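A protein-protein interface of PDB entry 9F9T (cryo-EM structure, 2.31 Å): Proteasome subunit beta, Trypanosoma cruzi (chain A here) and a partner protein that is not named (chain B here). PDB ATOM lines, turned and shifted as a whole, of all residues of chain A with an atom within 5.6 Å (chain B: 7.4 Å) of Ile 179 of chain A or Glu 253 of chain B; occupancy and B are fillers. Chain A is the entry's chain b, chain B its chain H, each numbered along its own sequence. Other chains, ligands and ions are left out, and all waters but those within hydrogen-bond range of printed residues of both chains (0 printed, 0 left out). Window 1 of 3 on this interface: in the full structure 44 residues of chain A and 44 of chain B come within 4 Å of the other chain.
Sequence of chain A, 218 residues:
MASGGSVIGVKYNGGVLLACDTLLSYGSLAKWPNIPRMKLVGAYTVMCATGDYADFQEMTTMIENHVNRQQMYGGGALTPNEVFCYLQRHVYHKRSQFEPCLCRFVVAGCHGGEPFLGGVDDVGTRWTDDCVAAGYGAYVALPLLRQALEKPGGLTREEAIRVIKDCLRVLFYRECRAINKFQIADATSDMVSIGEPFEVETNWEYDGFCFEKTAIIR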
ATOM      1  N   ASP A  21      15.990  21.914 -36.717  1.00  0.00           N
ATOM      2  CA  ASP A  21      16.073  20.837 -35.758  1.00  0.00           C
ATOM      3  C   ASP A  21      16.126  19.514 -36.509  1.00  0.00           C
ATOM      4  O   ASP A  21      15.970  19.508 -37.718  1.00  0.00           O
ATOM      5  CB  ASP A  21      14.944  20.835 -34.748  1.00  0.00           C
ATOM      6  CG  ASP A  21      13.627  20.419 -35.383  1.00  0.00           C
ATOM      7  OD1 ASP A  21      13.677  19.760 -36.493  1.00  0.00           O
ATOM      8  OD2 ASP A  21      12.531  20.771 -34.760  1.00  0.00           O
ATOM      9  N   THR A  22      16.366  18.446 -35.742  1.00  0.00           N
ATOM     10  CA  THR A  22      16.668  17.147 -36.299  1.00  0.00           C
ATOM     11  C   THR A  22      15.500  16.200 -36.119  1.00  0.00           C
ATOM     12  O   THR A  22      15.709  15.047 -35.850  1.00  0.00           O
ATOM     13  CB  THR A  22      17.920  16.601 -35.600  1.00  0.00           C
ATOM     14  OG1 THR A  22      17.727  16.538 -34.186  1.00  0.00           O
ATOM     15  CG2 THR A  22      19.156  17.427 -35.964  1.00  0.00           C
ATOM     16  N   LEU A  23      14.292  16.670 -36.219  1.00  0.00           N
ATOM     17  CA  LEU A  23      13.151  15.868 -35.895  1.00  0.00           C
ATOM     18  C   LEU A  23      12.229  15.699 -37.078  1.00  0.00           C
ATOM     19  O   LEU A  23      11.927  16.660 -37.740  1.00  0.00           O
ATOM     20  CB  LEU A  23      12.386  16.563 -34.770  1.00  0.00           C
ATOM     21  CG  LEU A  23      11.044  15.925 -34.397  1.00  0.00           C
ATOM     22  CD1 LEU A  23      11.187  14.643 -33.639  1.00  0.00           C
ATOM     23  CD2 LEU A  23      10.179  16.892 -33.591  1.00  0.00           C
ATOM     24  N   ALA A  30       6.455  12.499 -32.089  1.00  0.00           N
ATOM     25  CA  ALA A  30       7.846  12.767 -32.393  1.00  0.00           C
ATOM     26  C   ALA A  30       8.513  11.485 -32.687  1.00  0.00           C
ATOM     27  O   ALA A  30       8.835  10.807 -31.760  1.00  0.00           O
ATOM     28  CB  ALA A  30       8.534  13.420 -31.223  1.00  0.00           C
ATOM     29  N   PRO A  33      14.087  11.553 -33.647  1.00  0.00           N
ATOM     30  CA  PRO A  33      14.733  12.781 -33.150  1.00  0.00           C
ATOM     31  C   PRO A  33      16.132  12.985 -33.651  1.00  0.00           C
ATOM     32  O   PRO A  33      16.707  14.001 -33.342  1.00  0.00           O
ATOM     33  CB  PRO A  33      14.756  12.495 -31.656  1.00  0.00           C
ATOM     34  CG  PRO A  33      15.085  10.983 -31.601  1.00  0.00           C
ATOM     35  CD  PRO A  33      14.267  10.387 -32.723  1.00  0.00           C
ATOM     36  N   PHE A 172      11.483  26.234 -29.754  1.00  0.00           N
ATOM     37  CA  PHE A 172      11.445  25.197 -28.774  1.00  0.00           C
ATOM     38  C   PHE A 172      10.399  25.527 -27.724  1.00  0.00           C
ATOM     39  O   PHE A 172       9.682  24.624 -27.335  1.00  0.00           O
ATOM     40  CB  PHE A 172      12.819  24.994 -28.143  1.00  0.00           C
ATOM     41  CG  PHE A 172      12.760  23.909 -27.124  1.00  0.00           C
ATOM     42  CD1 PHE A 172      12.305  22.641 -27.482  1.00  0.00           C
ATOM     43  CD2 PHE A 172      12.979  24.168 -25.787  1.00  0.00           C
ATOM     44  CE1 PHE A 172      12.156  21.633 -26.527  1.00  0.00           C
ATOM     45  CE2 PHE A 172      12.886  23.142 -24.842  1.00  0.00           C
ATOM     46  CZ  PHE A 172      12.474  21.883 -25.207  1.00  0.00           C
ATOM     47  N   ARG A 177       5.646  20.714 -32.058  1.00  0.00           N
ATOM     48  CA  ARG A 177       6.320  19.580 -32.673  1.00  0.00           C
ATOM     49  C   ARG A 177       7.776  19.887 -32.984  1.00  0.00           C
ATOM     50  O   ARG A 177       8.170  20.014 -34.148  1.00  0.00           O
ATOM     51  CB  ARG A 177       5.608  19.250 -34.001  1.00  0.00           C
ATOM     52  CG  ARG A 177       4.204  18.750 -33.721  1.00  0.00           C
ATOM     53  CD  ARG A 177       3.353  18.534 -34.942  1.00  0.00           C
ATOM     54  NE  ARG A 177       2.009  18.327 -34.413  1.00  0.00           N
ATOM     55  CZ  ARG A 177       0.943  18.093 -35.160  1.00  0.00           C
ATOM     56  NH1 ARG A 177      -0.205  17.747 -34.608  1.00  0.00           N
ATOM     57  NH2 ARG A 177       1.049  18.184 -36.468  1.00  0.00           N
ATOM     58  N   ALA A 178       8.545  19.947 -31.935  1.00  0.00           N
ATOM     59  CA  ALA A 178       9.920  20.392 -31.978  1.00  0.00           C
ATOM     60  C   ALA A 178      10.712  19.667 -30.891  1.00  0.00           C
ATOM     61  O   ALA A 178      10.189  18.923 -30.071  1.00  0.00           O
ATOM     62  CB  ALA A 178       9.940  21.862 -31.701  1.00  0.00           C
ATOM     63  N   ILE A 179      11.996  19.876 -30.925  1.00  0.00           N
ATOM     64  CA  ILE A 179      12.863  19.367 -29.897  1.00  0.00           C
ATOM     65  C   ILE A 179      14.055  20.299 -29.775  1.00  0.00           C
ATOM     66  O   ILE A 179      14.437  20.930 -30.752  1.00  0.00           O
ATOM     67  CB  ILE A 179      13.491  18.006 -30.260  1.00  0.00           C
ATOM     68  CG1 ILE A 179      14.112  17.995 -31.645  1.00  0.00           C
ATOM     69  CG2 ILE A 179      12.557  16.851 -30.063  1.00  0.00           C
ATOM     70  CD1 ILE A 179      15.011  16.806 -31.748  1.00  0.00           C
ATOM     71  N   ASN A 180      14.749  20.145 -28.647  1.00  0.00           N
ATOM     72  CA  ASN A 180      15.856  21.006 -28.351  1.00  0.00           C
ATOM     73  C   ASN A 180      17.116  20.425 -28.924  1.00  0.00           C
ATOM     74  O   ASN A 180      17.957  19.982 -28.149  1.00  0.00           O
ATOM     75  CB  ASN A 180      16.023  21.279 -26.857  1.00  0.00           C
ATOM     76  CG  ASN A 180      16.920  22.464 -26.674  1.00  0.00           C
ATOM     77  OD1 ASN A 180      17.608  22.908 -27.570  1.00  0.00           O
ATOM     78  ND2 ASN A 180      16.934  23.008 -25.503  1.00  0.00           N
ATOM     79  N   LYS A 181      17.226  20.424 -30.249  1.00  0.00           N
ATOM     80  CA  LYS A 181      18.366  19.796 -30.891  1.00  0.00           C
ATOM     81  C   LYS A 181      18.465  20.226 -32.337  1.00  0.00           C
ATOM     82  O   LYS A 181      17.584  19.909 -33.103  1.00  0.00           O
ATOM     83  CB  LYS A 181      18.237  18.285 -30.937  1.00  0.00           C
ATOM     84  CG  LYS A 181      19.501  17.590 -31.413  1.00  0.00           C
ATOM     85  CD  LYS A 181      19.369  16.153 -31.121  1.00  0.00           C
ATOM     86  CE  LYS A 181      20.287  15.255 -31.903  1.00  0.00           C
ATOM     87  NZ  LYS A 181      19.708  13.897 -31.820  1.00  0.00           N
ATOM     88  N   PHE A 182      19.526  20.946 -32.678  1.00  0.00           N
ATOM     89  CA  PHE A 182      19.516  21.783 -33.856  1.00  0.00           C
ATOM     90  C   PHE A 182      20.859  21.706 -34.527  1.00  0.00           C
ATOM     91  O   PHE A 182      21.828  21.324 -33.958  1.00  0.00           O
ATOM     92  CB  PHE A 182      19.256  23.242 -33.509  1.00  0.00           C
ATOM     93  CG  PHE A 182      18.017  23.561 -32.720  1.00  0.00           C
ATOM     94  CD1 PHE A 182      16.790  23.747 -33.348  1.00  0.00           C
ATOM     95  CD2 PHE A 182      18.055  23.701 -31.351  1.00  0.00           C
ATOM     96  CE1 PHE A 182      15.618  24.003 -32.619  1.00  0.00           C
ATOM     97  CE2 PHE A 182      16.888  24.005 -30.631  1.00  0.00           C
ATOM     98  CZ  PHE A 182      15.669  24.120 -31.266  1.00  0.00           C
ATOM     99  N   SER B 219       8.130  13.354 -24.062  1.00  0.00           N
ATOM    100  CA  SER B 219       9.172  13.372 -25.069  1.00  0.00           C
ATOM    101  C   SER B 219       8.704  12.866 -26.423  1.00  0.00           C
ATOM    102  O   SER B 219       9.449  12.959 -27.376  1.00  0.00           O
ATOM    103  CB  SER B 219      10.322  12.490 -24.593  1.00  0.00           C
ATOM    104  OG  SER B 219      10.853  13.057 -23.378  1.00  0.00           O
ATOM    105  N   TRP B 245      12.034  21.715 -17.301  1.00  0.00           N
ATOM    106  CA  TRP B 245      12.375  20.857 -18.420  1.00  0.00           C
ATOM    107  C   TRP B 245      13.876  20.582 -18.433  1.00  0.00           C
ATOM    108  O   TRP B 245      14.273  19.536 -18.901  1.00  0.00           O
ATOM    109  CB  TRP B 245      11.920  21.453 -19.786  1.00  0.00           C
ATOM    110  CG  TRP B 245      12.260  20.496 -20.903  1.00  0.00           C
ATOM    111  CD1 TRP B 245      11.558  19.378 -21.263  1.00  0.00           C
ATOM    112  CD2 TRP B 245      13.501  20.435 -21.658  1.00  0.00           C
ATOM    113  NE1 TRP B 245      12.258  18.650 -22.207  1.00  0.00           N
ATOM    114  CE2 TRP B 245      13.448  19.293 -22.478  1.00  0.00           C
ATOM    115  CE3 TRP B 245      14.618  21.244 -21.758  1.00  0.00           C
ATOM    116  CZ2 TRP B 245      14.488  18.949 -23.355  1.00  0.00           C
ATOM    117  CZ3 TRP B 245      15.660  20.895 -22.613  1.00  0.00           C
ATOM    118  CH2 TRP B 245      15.611  19.736 -23.379  1.00  0.00           C
ATOM    119  N   THR B 248      14.530  17.472 -16.398  1.00  0.00           N
ATOM    120  CA  THR B 248      13.696  16.320 -16.672  1.00  0.00           C
ATOM    121  C   THR B 248      14.503  15.030 -16.618  1.00  0.00           C
ATOM    122  O   THR B 248      15.608  14.949 -17.095  1.00  0.00           O
ATOM    123  CB  THR B 248      12.941  16.456 -17.992  1.00  0.00           C
ATOM    124  OG1 THR B 248      11.902  15.479 -18.090  1.00  0.00           O
ATOM    125  CG2 THR B 248      13.829  16.355 -19.216  1.00  0.00           C
ATOM    126  N   TYR B 250      14.030  12.371 -18.266  1.00  0.00           N
ATOM    127  CA  TYR B 250      14.238  11.703 -19.546  1.00  0.00           C
ATOM    128  C   TYR B 250      13.936  12.732 -20.614  1.00  0.00           C
ATOM    129  O   TYR B 250      12.946  13.414 -20.500  1.00  0.00           O
ATOM    130  CB  TYR B 250      13.381  10.428 -19.741  1.00  0.00           C
ATOM    131  CG  TYR B 250      13.631   9.813 -21.088  1.00  0.00           C
ATOM    132  CD1 TYR B 250      14.790   9.084 -21.286  1.00  0.00           C
ATOM    133  CD2 TYR B 250      12.828  10.112 -22.198  1.00  0.00           C
ATOM    134  CE1 TYR B 250      15.084   8.580 -22.534  1.00  0.00           C
ATOM    135  CE2 TYR B 250      13.162   9.645 -23.468  1.00  0.00           C
ATOM    136  CZ  TYR B 250      14.321   8.909 -23.633  1.00  0.00           C
ATOM    137  OH  TYR B 250      14.713   8.389 -24.806  1.00  0.00           O
ATOM    138  N   CYS B 251      14.806  12.847 -21.596  1.00  0.00           N
ATOM    139  CA  CYS B 251      14.428  13.317 -22.916  1.00  0.00           C
ATOM    140  C   CYS B 251      15.280  12.701 -24.000  1.00  0.00           C
ATOM    141  O   CYS B 251      16.453  12.400 -23.765  1.00  0.00           O
ATOM    142  CB  CYS B 251      14.640  14.823 -23.084  1.00  0.00           C
ATOM    143  SG  CYS B 251      16.253  15.399 -22.518  1.00  0.00           S
ATOM    144  N   MET B 252      14.712  12.655 -25.198  1.00  0.00           N
ATOM    145  CA  MET B 252      15.417  12.090 -26.340  1.00  0.00           C
ATOM    146  C   MET B 252      16.653  12.912 -26.716  1.00  0.00           C
ATOM    147  O   MET B 252      17.593  12.347 -27.279  1.00  0.00           O
ATOM    148  CB  MET B 252      14.486  11.999 -27.561  1.00  0.00           C
ATOM    149  CG  MET B 252      13.388  10.970 -27.377  1.00  0.00           C
ATOM    150  SD  MET B 252      12.445  10.666 -28.905  1.00  0.00           S
ATOM    151  CE  MET B 252      11.662  12.245 -29.254  1.00  0.00           C
ATOM    152  N   GLU B 253      16.637  14.228 -26.424  1.00  0.00           N
ATOM    153  CA  GLU B 253      17.759  15.123 -26.693  1.00  0.00           C
ATOM    154  C   GLU B 253      18.992  14.706 -25.909  1.00  0.00           C
ATOM    155  O   GLU B 253      20.089  14.952 -26.360  1.00  0.00           O
ATOM    156  CB  GLU B 253      17.453  16.597 -26.389  1.00  0.00           C
ATOM    157  CG  GLU B 253      16.261  17.201 -27.156  1.00  0.00           C
ATOM    158  CD  GLU B 253      14.844  17.068 -26.538  1.00  0.00           C
ATOM    159  OE1 GLU B 253      14.569  16.034 -25.860  1.00  0.00           O
ATOM    160  OE2 GLU B 253      13.973  17.963 -26.771  1.00  0.00           O
ATOM    161  N   LYS B 254      18.832  14.069 -24.744  1.00  0.00           N
ATOM    162  CA  LYS B 254      19.970  13.755 -23.891  1.00  0.00           C
ATOM    163  C   LYS B 254      20.246  12.266 -23.818  1.00  0.00           C
ATOM    164  O   LYS B 254      21.256  11.885 -23.228  1.00  0.00           O
ATOM    165  CB  LYS B 254      19.808  14.389 -22.504  1.00  0.00           C
ATOM    166  CG  LYS B 254      20.042  15.898 -22.553  1.00  0.00           C
ATOM    167  CD  LYS B 254      19.433  16.728 -21.456  1.00  0.00           C
ATOM    168  CE  LYS B 254      19.791  18.194 -21.613  1.00  0.00           C
ATOM    169  NZ  LYS B 254      19.160  19.054 -20.571  1.00  0.00           N
ATOM    170  N   ASP B 255      19.389  11.465 -24.454  1.00  0.00           N
ATOM    171  CA  ASP B 255      19.512  10.020 -24.469  1.00  0.00           C
ATOM    172  C   ASP B 255      20.576   9.625 -25.461  1.00  0.00           C
ATOM    173  O   ASP B 255      20.446   9.941 -26.642  1.00  0.00           O
ATOM    174  CB  ASP B 255      18.199   9.320 -24.865  1.00  0.00           C
ATOM    175  CG  ASP B 255      18.252   7.801 -24.889  1.00  0.00           C
ATOM    176  OD1 ASP B 255      19.348   7.268 -24.777  1.00  0.00           O
ATOM    177  OD2 ASP B 255      17.181   7.169 -24.993  1.00  0.00           O
ATOM    178  N   PRO B 256      21.658   8.954 -25.014  1.00  0.00           N
ATOM    179  CA  PRO B 256      22.791   8.615 -25.893  1.00  0.00           C
ATOM    180  C   PRO B 256      22.534   7.735 -27.125  1.00  0.00           C
ATOM    181  O   PRO B 256      23.278   7.783 -28.088  1.00  0.00           O
ATOM    182  CB  PRO B 256      23.750   7.829 -24.991  1.00  0.00           C
ATOM    183  CG  PRO B 256      23.327   8.163 -23.590  1.00  0.00           C
ATOM    184  CD  PRO B 256      21.850   8.519 -23.622  1.00  0.00           C
ATOM    185  N   TYR B 258      20.257   8.352 -29.164  1.00  0.00           N
ATOM    186  CA  TYR B 258      19.839   9.203 -30.270  1.00  0.00           C
ATOM    187  C   TYR B 258      20.853  10.297 -30.582  1.00  0.00           C
ATOM    188  O   TYR B 258      20.543  11.221 -31.307  1.00  0.00           O
ATOM    189  CB  TYR B 258      18.466   9.783 -29.957  1.00  0.00           C
ATOM    190  CG  TYR B 258      17.368   8.772 -29.627  1.00  0.00           C
ATOM    191  CD1 TYR B 258      17.012   7.777 -30.515  1.00  0.00           C
ATOM    192  CD2 TYR B 258      16.655   8.859 -28.448  1.00  0.00           C
ATOM    193  CE1 TYR B 258      16.034   6.844 -30.212  1.00  0.00           C
ATOM    194  CE2 TYR B 258      15.647   7.953 -28.131  1.00  0.00           C
ATOM    195  CZ  TYR B 258      15.317   6.950 -29.031  1.00  0.00           C
ATOM    196  OH  TYR B 258      14.324   6.053 -28.752  1.00  0.00           O
ATOM    197  N   ARG B 259      22.087  10.170 -30.101  1.00  0.00           N
ATOM    198  CA  ARG B 259      23.051  11.233 -30.294  1.00  0.00           C
ATOM    199  C   ARG B 259      23.520  11.263 -31.755  1.00  0.00           C
ATOM    200  O   ARG B 259      23.432  12.311 -32.402  1.00  0.00           O
ATOM    201  CB  ARG B 259      24.204  11.047 -29.306  1.00  0.00           C
ATOM    202  CG  ARG B 259      25.041  12.297 -29.100  1.00  0.00           C
ATOM    203  CD  ARG B 259      26.145  12.115 -28.074  1.00  0.00           C
ATOM    204  NE  ARG B 259      26.899  10.893 -28.345  1.00  0.00           N
ATOM    205  CZ  ARG B 259      27.590  10.662 -29.462  1.00  0.00           C
ATOM    206  NH1 ARG B 259      27.771  11.632 -30.345  1.00  0.00           N
ATOM    207  NH2 ARG B 259      28.126   9.472 -29.675  1.00  0.00           N
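O of Tyr 258 of chain B is in hydrogen-bond range of NZ of Lys 181 of chain A (2.8 Å).
The backbone NH (N) of Asn 180 of chain A sits at hydrogen-bond distance from the side-chain carboxylate (OE2) of Glu 253 of chain B, at 3.0 Å.
The backbone carbonyl oxygen of Pro 33 of chain A sits at hydrogen-bond distance from the side-chain amino group of Lys 181 of chain A (3.4 Å).
The backbone carbonyl oxygen of Pro 33 of chain A is in hydrogen-bond range of the side-chain hydroxyl of Thr 22 of chain A (2.9 Å).
The side-chain sulfur (SG) of Cys 251 of chain B lies close to the side-chain carboxylate (OE1) of Glu 253 of chain B (3.8 Å).
The backbone NH (N) of Thr 22 of chain A sits at hydrogen-bond distance from the backbone carbonyl oxygen (O) of Lys 181 of chain A (3.3 Å).
Among the printed residues, pairs that only touch across the chains: Ile 179 of chain A with Glu 253 of chain B, Pro 33 of chain A with Tyr 258 of chain B, Pro 33 of chain A with Met 252 of chain B, Asn 180 of chain A with Trp 245 of chain B, Ala 30 of chain A with Met 252 of chain B, Phe 172 of chain A with Trp 245 of chain B and Ala 30 of chain A with Ser 219 of chain B.
Asp 21 of chain A touches none of the printed residues of chain B.
Ile 179 of chain A touches one residue of chain B.
Of the printed residues of chain A, Ser 219 of chain B touches Ala 30.
Thr 248 of chain B touches none of the printed residues of chain A.
Printed residues of chain A within 4 Å of Met 252 of chain B: Ala 30 and Pro 33.
The nearest residue of chain B that does not touch Ile 179 of chain A is Met 252 of chain B (4.8 Å).
Printed residues of chain A that touch a printed residue of chain B: Ala 30, Pro 33, Phe 172, Ile 179, Asn 180 and Lys 181.
Hydrophobic or aromatic side chains of chain A that line the printed part of chain B: Ala 30, Pro 33, Phe 172 and Ile 179.
Of the 12 printed residues of chain B, 5 touch a printed residue of chain A.
Hydrophobic or aromatic side chains of chain B within 4 Å of the printed part of chain A: Trp 245, Met 252 and Tyr 258.
Among the printed residues, 9 pairs touch across the chains.
Among the printed residues, no Asp or Glu carboxylate lies within 4 Å of a Lys or Arg side-chain nitrogen of the other chain.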
